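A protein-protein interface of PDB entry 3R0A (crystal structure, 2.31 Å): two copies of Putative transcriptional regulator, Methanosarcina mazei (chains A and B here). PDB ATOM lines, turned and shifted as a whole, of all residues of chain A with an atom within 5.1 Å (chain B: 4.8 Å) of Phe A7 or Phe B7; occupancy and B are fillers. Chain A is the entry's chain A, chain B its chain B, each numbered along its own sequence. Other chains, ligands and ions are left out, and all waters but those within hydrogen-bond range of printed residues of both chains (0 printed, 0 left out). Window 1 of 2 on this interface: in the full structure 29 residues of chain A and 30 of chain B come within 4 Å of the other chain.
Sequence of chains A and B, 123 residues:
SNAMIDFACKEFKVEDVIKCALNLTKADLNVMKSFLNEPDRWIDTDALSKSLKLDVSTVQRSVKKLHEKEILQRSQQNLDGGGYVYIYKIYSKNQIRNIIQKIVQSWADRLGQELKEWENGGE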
ATOM      1  N   ILE A   5       9.264  25.934   5.941  1.00  0.00           N
ATOM      2  CA  ILE A   5       8.231  26.824   6.438  1.00  0.00           C
ATOM      3  C   ILE A   5       6.837  26.206   6.313  1.00  0.00           C
ATOM      4  O   ILE A   5       6.576  25.321   5.484  1.00  0.00           O
ATOM      5  CB  ILE A   5       8.255  28.227   5.778  1.00  0.00           C
ATOM      6  CG1 ILE A   5       8.390  28.131   4.254  1.00  0.00           C
ATOM      7  CG2 ILE A   5       9.372  29.049   6.343  1.00  0.00           C
ATOM      8  CD1 ILE A   5       7.059  28.095   3.517  1.00  0.00           C
ATOM      9  N   ASP A   6       5.946  26.688   7.166  1.00  0.00           N
ATOM     10  CA  ASP A   6       4.543  26.375   7.037  1.00  0.00           C
ATOM     11  C   ASP A   6       3.779  27.605   6.530  1.00  0.00           C
ATOM     12  O   ASP A   6       4.006  28.724   6.979  1.00  0.00           O
ATOM     13  CB  ASP A   6       3.972  25.846   8.354  1.00  0.00           C
ATOM     14  CG  ASP A   6       4.116  26.826   9.468  1.00  0.00           C
ATOM     15  OD1 ASP A   6       5.197  26.853  10.080  1.00  0.00           O
ATOM     16  OD2 ASP A   6       3.143  27.570   9.721  1.00  0.00           O
ATOM     17  N   PHE A   7       2.908  27.362   5.555  1.00  0.00           N
ATOM     18  CA  PHE A   7       1.965  28.352   5.086  1.00  0.00           C
ATOM     19  C   PHE A   7       0.615  27.673   5.040  1.00  0.00           C
ATOM     20  O   PHE A   7       0.506  26.520   4.576  1.00  0.00           O
ATOM     21  CB  PHE A   7       2.345  28.837   3.688  1.00  0.00           C
ATOM     22  CG  PHE A   7       1.606  30.049   3.274  1.00  0.00           C
ATOM     23  CD1 PHE A   7       2.175  31.305   3.443  1.00  0.00           C
ATOM     24  CD2 PHE A   7       0.307  29.950   2.788  1.00  0.00           C
ATOM     25  CE1 PHE A   7       1.485  32.451   3.094  1.00  0.00           C
ATOM     26  CE2 PHE A   7      -0.412  31.095   2.444  1.00  0.00           C
ATOM     27  CZ  PHE A   7       0.192  32.359   2.586  1.00  0.00           C
ATOM     28  N   ALA A   8      -0.419  28.372   5.498  1.00  0.00           N
ATOM     29  CA  ALA A   8      -1.768  27.783   5.578  1.00  0.00           C
ATOM     30  C   ALA A   8      -1.753  26.327   6.079  1.00  0.00           C
ATOM     31  O   ALA A   8      -2.268  25.424   5.408  1.00  0.00           O
ATOM     32  CB  ALA A   8      -2.449  27.858   4.243  1.00  0.00           C
ATOM     33  N   CYS A   9      -1.123  26.112   7.236  1.00  0.00           N
ATOM     34  CA  CYS A   9      -1.036  24.781   7.878  1.00  0.00           C
ATOM     35  C   CYS A   9      -0.423  23.646   7.021  1.00  0.00           C
ATOM     36  O   CYS A   9      -0.709  22.462   7.240  1.00  0.00           O
ATOM     37  CB  CYS A   9      -2.409  24.367   8.412  1.00  0.00           C
ATOM     38  SG  CYS A   9      -3.104  25.474   9.672  1.00  0.00           S
ATOM     39  N   LYS A  10       0.418  23.990   6.046  1.00  0.00           N
ATOM     40  CA  LYS A  10       1.172  22.959   5.320  1.00  0.00           C
ATOM     41  C   LYS A  10       2.663  23.274   5.265  1.00  0.00           C
ATOM     42  O   LYS A  10       3.064  24.436   5.325  1.00  0.00           O
ATOM     43  CB  LYS A  10       0.614  22.723   3.916  1.00  0.00           C
ATOM     44  CG  LYS A  10      -0.370  21.537   3.805  1.00  0.00           C
ATOM     45  CD  LYS A  10      -1.043  21.447   2.417  1.00  0.00           C
ATOM     46  CE  LYS A  10      -2.463  20.824   2.492  1.00  0.00           C
ATOM     47  NZ  LYS A  10      -3.073  20.510   1.127  1.00  0.00           N
ATOM     48  N   PHE A  12       6.379  23.519   3.622  1.00  0.00           N
ATOM     49  CA  PHE A  12       7.094  23.777   2.384  1.00  0.00           C
ATOM     50  C   PHE A  12       8.573  23.895   2.708  1.00  0.00           C
ATOM     51  O   PHE A  12       8.928  24.460   3.741  1.00  0.00           O
ATOM     52  CB  PHE A  12       6.633  25.103   1.735  1.00  0.00           C
ATOM     53  CG  PHE A  12       5.143  25.188   1.441  1.00  0.00           C
ATOM     54  CD1 PHE A  12       4.669  24.987   0.138  1.00  0.00           C
ATOM     55  CD2 PHE A  12       4.237  25.514   2.438  1.00  0.00           C
ATOM     56  CE1 PHE A  12       3.304  25.084  -0.169  1.00  0.00           C
ATOM     57  CE2 PHE A  12       2.848  25.596   2.156  1.00  0.00           C
ATOM     58  CZ  PHE A  12       2.386  25.383   0.838  1.00  0.00           C
ATOM     59  N   VAL A 104       4.395  36.704  -3.751  1.00  0.00           N
ATOM     60  CA  VAL A 104       3.779  35.998  -2.636  1.00  0.00           C
ATOM     61  C   VAL A 104       2.518  36.737  -2.226  1.00  0.00           C
ATOM     62  O   VAL A 104       1.538  36.132  -1.833  1.00  0.00           O
ATOM     63  CB  VAL A 104       4.725  35.847  -1.459  1.00  0.00           C
ATOM     64  CG1 VAL A 104       3.933  35.685  -0.123  1.00  0.00           C
ATOM     65  CG2 VAL A 104       5.706  34.702  -1.704  1.00  0.00           C
ATOM     66  N   TRP A 107      -0.311  35.857  -4.430  1.00  0.00           N
ATOM     67  CA  TRP A 107      -0.909  34.560  -4.036  1.00  0.00           C
ATOM     68  C   TRP A 107      -1.937  34.764  -2.933  1.00  0.00           C
ATOM     69  O   TRP A 107      -2.985  34.102  -2.908  1.00  0.00           O
ATOM     70  CB  TRP A 107       0.124  33.606  -3.481  1.00  0.00           C
ATOM     71  CG  TRP A 107       1.119  33.041  -4.416  1.00  0.00           C
ATOM     72  CD1 TRP A 107       1.039  32.968  -5.774  1.00  0.00           C
ATOM     73  CD2 TRP A 107       2.356  32.414  -4.044  1.00  0.00           C
ATOM     74  NE1 TRP A 107       2.169  32.356  -6.272  1.00  0.00           N
ATOM     75  CE2 TRP A 107       2.987  31.997  -5.231  1.00  0.00           C
ATOM     76  CE3 TRP A 107       2.997  32.183  -2.827  1.00  0.00           C
ATOM     77  CZ2 TRP A 107       4.242  31.364  -5.233  1.00  0.00           C
ATOM     78  CZ3 TRP A 107       4.234  31.534  -2.833  1.00  0.00           C
ATOM     79  CH2 TRP A 107       4.830  31.128  -4.024  1.00  0.00           C
ATOM     80  N   ALA A 108      -1.590  35.661  -2.013  1.00  0.00           N
ATOM     81  CA  ALA A 108      -2.433  36.042  -0.877  1.00  0.00           C
ATOM     82  C   ALA A 108      -3.679  36.776  -1.352  1.00  0.00           C
ATOM     83  O   ALA A 108      -4.785  36.394  -0.995  1.00  0.00           O
ATOM     84  CB  ALA A 108      -1.650  36.939   0.056  1.00  0.00           C
ATOM     85  N   LEU A 111      -6.085  34.217  -3.135  1.00  0.00           N
ATOM     86  CA  LEU A 111      -6.763  33.279  -2.231  1.00  0.00           C
ATOM     87  C   LEU A 111      -7.886  34.056  -1.561  1.00  0.00           C
ATOM     88  O   LEU A 111      -8.916  33.489  -1.230  1.00  0.00           O
ATOM     89  CB  LEU A 111      -5.794  32.635  -1.217  1.00  0.00           C
ATOM     90  CG  LEU A 111      -6.247  31.866   0.047  1.00  0.00           C
ATOM     91  CD1 LEU A 111      -7.179  30.689  -0.230  1.00  0.00           C
ATOM     92  CD2 LEU A 111      -5.050  31.390   0.898  1.00  0.00           C
ATOM     93  N   ILE B   5      -8.178  25.398  -4.351  1.00  0.00           N
ATOM     94  CA  ILE B   5      -7.330  26.562  -4.578  1.00  0.00           C
ATOM     95  C   ILE B   5      -5.841  26.173  -4.471  1.00  0.00           C
ATOM     96  O   ILE B   5      -5.482  25.171  -3.836  1.00  0.00           O
ATOM     97  CB  ILE B   5      -7.737  27.761  -3.667  1.00  0.00           C
ATOM     98  CG1 ILE B   5      -7.203  29.102  -4.201  1.00  0.00           C
ATOM     99  CG2 ILE B   5      -7.324  27.519  -2.228  1.00  0.00           C
ATOM    100  CD1 ILE B   5      -7.465  29.332  -5.701  1.00  0.00           C
ATOM    101  N   ASP B   6      -5.000  26.956  -5.144  1.00  0.00           N
ATOM    102  CA  ASP B   6      -3.581  26.653  -5.302  1.00  0.00           C
ATOM    103  C   ASP B   6      -2.744  27.823  -4.833  1.00  0.00           C
ATOM    104  O   ASP B   6      -2.799  28.947  -5.368  1.00  0.00           O
ATOM    105  CB  ASP B   6      -3.220  26.231  -6.737  1.00  0.00           C
ATOM    106  CG  ASP B   6      -3.754  27.193  -7.802  1.00  0.00           C
ATOM    107  OD1 ASP B   6      -3.499  28.423  -7.706  1.00  0.00           O
ATOM    108  OD2 ASP B   6      -4.423  26.705  -8.751  1.00  0.00           O
ATOM    109  N   PHE B   7      -1.980  27.527  -3.792  1.00  0.00           N
ATOM    110  CA  PHE B   7      -1.110  28.473  -3.184  1.00  0.00           C
ATOM    111  C   PHE B   7       0.250  27.819  -3.202  1.00  0.00           C
ATOM    112  O   PHE B   7       0.389  26.630  -2.837  1.00  0.00           O
ATOM    113  CB  PHE B   7      -1.547  28.736  -1.749  1.00  0.00           C
ATOM    114  CG  PHE B   7      -1.001  30.003  -1.195  1.00  0.00           C
ATOM    115  CD1 PHE B   7      -1.785  31.153  -1.172  1.00  0.00           C
ATOM    116  CD2 PHE B   7       0.318  30.067  -0.742  1.00  0.00           C
ATOM    117  CE1 PHE B   7      -1.279  32.360  -0.676  1.00  0.00           C
ATOM    118  CE2 PHE B   7       0.858  31.278  -0.249  1.00  0.00           C
ATOM    119  CZ  PHE B   7       0.053  32.427  -0.218  1.00  0.00           C
ATOM    120  N   ALA B   8       1.246  28.601  -3.619  1.00  0.00           N
ATOM    121  CA  ALA B   8       2.635  28.152  -3.730  1.00  0.00           C
ATOM    122  C   ALA B   8       2.743  26.756  -4.311  1.00  0.00           C
ATOM    123  O   ALA B   8       3.404  25.895  -3.725  1.00  0.00           O
ATOM    124  CB  ALA B   8       3.349  28.225  -2.374  1.00  0.00           C
ATOM    125  N   CYS B   9       2.052  26.528  -5.433  1.00  0.00           N
ATOM    126  CA  CYS B   9       2.272  25.325  -6.223  1.00  0.00           C
ATOM    127  C   CYS B   9       1.907  24.096  -5.395  1.00  0.00           C
ATOM    128  O   CYS B   9       2.464  23.007  -5.594  1.00  0.00           O
ATOM    129  CB  CYS B   9       3.761  25.265  -6.663  1.00  0.00           C
ATOM    130  SG  CYS B   9       4.289  26.589  -7.809  1.00  0.00           S
ATOM    131  N   LYS B  10       1.014  24.295  -4.425  1.00  0.00           N
ATOM    132  CA  LYS B  10       0.368  23.193  -3.705  1.00  0.00           C
ATOM    133  C   LYS B  10      -1.136  23.362  -3.621  1.00  0.00           C
ATOM    134  O   LYS B  10      -1.654  24.473  -3.740  1.00  0.00           O
ATOM    135  CB  LYS B  10       0.977  22.959  -2.325  1.00  0.00           C
ATOM    136  CG  LYS B  10       2.183  22.012  -2.397  1.00  0.00           C
ATOM    137  CD  LYS B  10       2.960  21.867  -1.093  1.00  0.00           C
ATOM    138  CE  LYS B  10       2.145  21.166  -0.017  1.00  0.00           C
ATOM    139  NZ  LYS B  10       1.535  22.177   0.873  1.00  0.00           N
ATOM    140  N   PHE B  12      -4.875  23.327  -2.239  1.00  0.00           N
ATOM    141  CA  PHE B  12      -5.645  23.574  -0.994  1.00  0.00           C
ATOM    142  C   PHE B  12      -7.174  23.451  -1.130  1.00  0.00           C
ATOM    143  O   PHE B  12      -7.808  24.135  -1.950  1.00  0.00           O
ATOM    144  CB  PHE B  12      -5.311  24.964  -0.391  1.00  0.00           C
ATOM    145  CG  PHE B  12      -3.926  25.067   0.184  1.00  0.00           C
ATOM    146  CD1 PHE B  12      -3.701  24.805   1.530  1.00  0.00           C
ATOM    147  CD2 PHE B  12      -2.843  25.414  -0.629  1.00  0.00           C
ATOM    148  CE1 PHE B  12      -2.432  24.895   2.078  1.00  0.00           C
ATOM    149  CE2 PHE B  12      -1.561  25.509  -0.102  1.00  0.00           C
ATOM    150  CZ  PHE B  12      -1.342  25.250   1.261  1.00  0.00           C
ATOM    151  N   VAL B 104      -4.633  35.714   6.588  1.00  0.00           N
ATOM    152  CA  VAL B 104      -3.894  35.385   5.361  1.00  0.00           C
ATOM    153  C   VAL B 104      -2.786  36.413   5.108  1.00  0.00           C
ATOM    154  O   VAL B 104      -1.679  36.065   4.760  1.00  0.00           O
ATOM    155  CB  VAL B 104      -4.814  35.383   4.111  1.00  0.00           C
ATOM    156  CG1 VAL B 104      -3.977  35.267   2.826  1.00  0.00           C
ATOM    157  CG2 VAL B 104      -5.849  34.243   4.185  1.00  0.00           C
ATOM    158  N   TRP B 107       0.200  35.665   7.218  1.00  0.00           N
ATOM    159  CA  TRP B 107       0.916  34.479   6.714  1.00  0.00           C
ATOM    160  C   TRP B 107       1.894  34.909   5.633  1.00  0.00           C
ATOM    161  O   TRP B 107       3.056  34.477   5.610  1.00  0.00           O
ATOM    162  CB  TRP B 107      -0.051  33.495   6.083  1.00  0.00           C
ATOM    163  CG  TRP B 107      -1.025  32.819   7.000  1.00  0.00           C
ATOM    164  CD1 TRP B 107      -0.991  32.778   8.375  1.00  0.00           C
ATOM    165  CD2 TRP B 107      -2.151  32.032   6.602  1.00  0.00           C
ATOM    166  NE1 TRP B 107      -2.045  32.043   8.852  1.00  0.00           N
ATOM    167  CE2 TRP B 107      -2.771  31.565   7.785  1.00  0.00           C
ATOM    168  CE3 TRP B 107      -2.687  31.663   5.362  1.00  0.00           C
ATOM    169  CZ2 TRP B 107      -3.912  30.757   7.763  1.00  0.00           C
ATOM    170  CZ3 TRP B 107      -3.838  30.869   5.339  1.00  0.00           C
ATOM    171  CH2 TRP B 107      -4.420  30.405   6.538  1.00  0.00           C
ATOM    172  N   ALA B 108       1.418  35.767   4.739  1.00  0.00           N
ATOM    173  CA  ALA B 108       2.261  36.306   3.660  1.00  0.00           C
ATOM    174  C   ALA B 108       3.421  37.145   4.199  1.00  0.00           C
ATOM    175  O   ALA B 108       4.529  37.063   3.666  1.00  0.00           O
ATOM    176  CB  ALA B 108       1.440  37.119   2.675  1.00  0.00           C
ATOM    177  N   LEU B 111       6.082  34.566   5.884  1.00  0.00           N
ATOM    178  CA  LEU B 111       6.812  33.930   4.768  1.00  0.00           C
ATOM    179  C   LEU B 111       7.795  34.959   4.168  1.00  0.00           C
ATOM    180  O   LEU B 111       8.918  34.626   3.783  1.00  0.00           O
ATOM    181  CB  LEU B 111       5.826  33.450   3.685  1.00  0.00           C
ATOM    182  CG  LEU B 111       6.020  32.170   2.836  1.00  0.00           C
ATOM    183  CD1 LEU B 111       5.136  32.198   1.579  1.00  0.00           C
ATOM    184  CD2 LEU B 111       7.439  31.834   2.453  1.00  0.00           C
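The backbone NH (N) of Phe A12 is in hydrogen-bond range of the backbone carbonyl oxygen (O) of Ile A5 (2.6 Å).
O of Ile B5 sits at hydrogen-bond distance from N of Phe B12 (2.5 Å).
Among the printed residues, pairs that only touch across the chains: Ile A5 with Leu B111 (3.9 Å), Phe A7 with Phe B7 (2.8 Å), Phe A7 with Trp B107 (3.5 Å), Phe A7 with Ala B108 (3.7 Å), Phe A7 with Leu B111 (3.6 Å), Ala A8 with Phe B12 (3.4 Å), Ala A8 with Trp B107 (3.5 Å), Lys A10 with Lys B10 (3.1 Å), Lys A10 with Phe B12 (3.7 Å), Phe A12 with Ala B8 (3.6 Å), Phe A12 with Lys B10 (3.3 Å), Phe A12 with Phe B12 (3.8 Å), Trp A107 with Phe B7 (3.3 Å), Trp A107 with Ala B8 (3.5 Å), Ala A108 with Phe B7 (3.6 Å), Ala A108 with Val B104 (3.99 Å), Leu A111 with Ile B5 (3.7 Å) and Leu A111 with Phe B7 (3.9 Å).
Of the printed residues of chain B, Phe A7 touches Phe B7 (2.8 Å), Trp B107 (3.5 Å), Ala B108 (3.7 Å) and Leu B111 (3.6 Å).
Cys A9 touches none of the printed residues of chain B.
Printed residues of chain B within 4 Å of Lys A10: Lys B10 and Phe B12.
Of the printed residues of chain B, Trp A107 touches Phe B7 (3.3 Å) and Ala B8 (3.5 Å).
Of the printed residues of chain A, Ile B5 touches Leu A111.
Of the printed residues of chain A, Ala B8 touches Phe A12 and Trp A107.
Of the printed residues of chain A, Val B104 touches Ala A108.
The nearest residue of chain A that does not touch Phe B7 is Phe A12 (4.2 Å).
Of the 11 printed residues of chain B, 9 touch a printed residue of chain A.
Hydrophobic or aromatic side chains of chain B within 4 Å of the printed part of chain A: Ile B5, Phe B7, Ala B8, Phe B12, Val B104, Trp B107 and Leu B111.
Hydrophobic or aromatic side chains of chain A that line the printed part of chain B: Ile A5, Phe A7, Ala A8, Phe A12, Trp A107, Ala A108 and Leu A111.
Phe A7 touches Trp B107, and with the chains exchanged Trp A107 touches Phe B7.
Phe A7 touches Ala B108, and with the chains exchanged Ala A108 touches Phe B7.
Ala A8 touches Trp B107, and with the chains exchanged Trp A107 touches Ala B8.
Ala A108 touches Val B104, but with the chains exchanged Val A104 does not touch Ala B108 (4.01 Å).
Positions printed for both chains: 5, 6, 7, 8, 9, 10, 12, 104, 107, 108 and 111.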
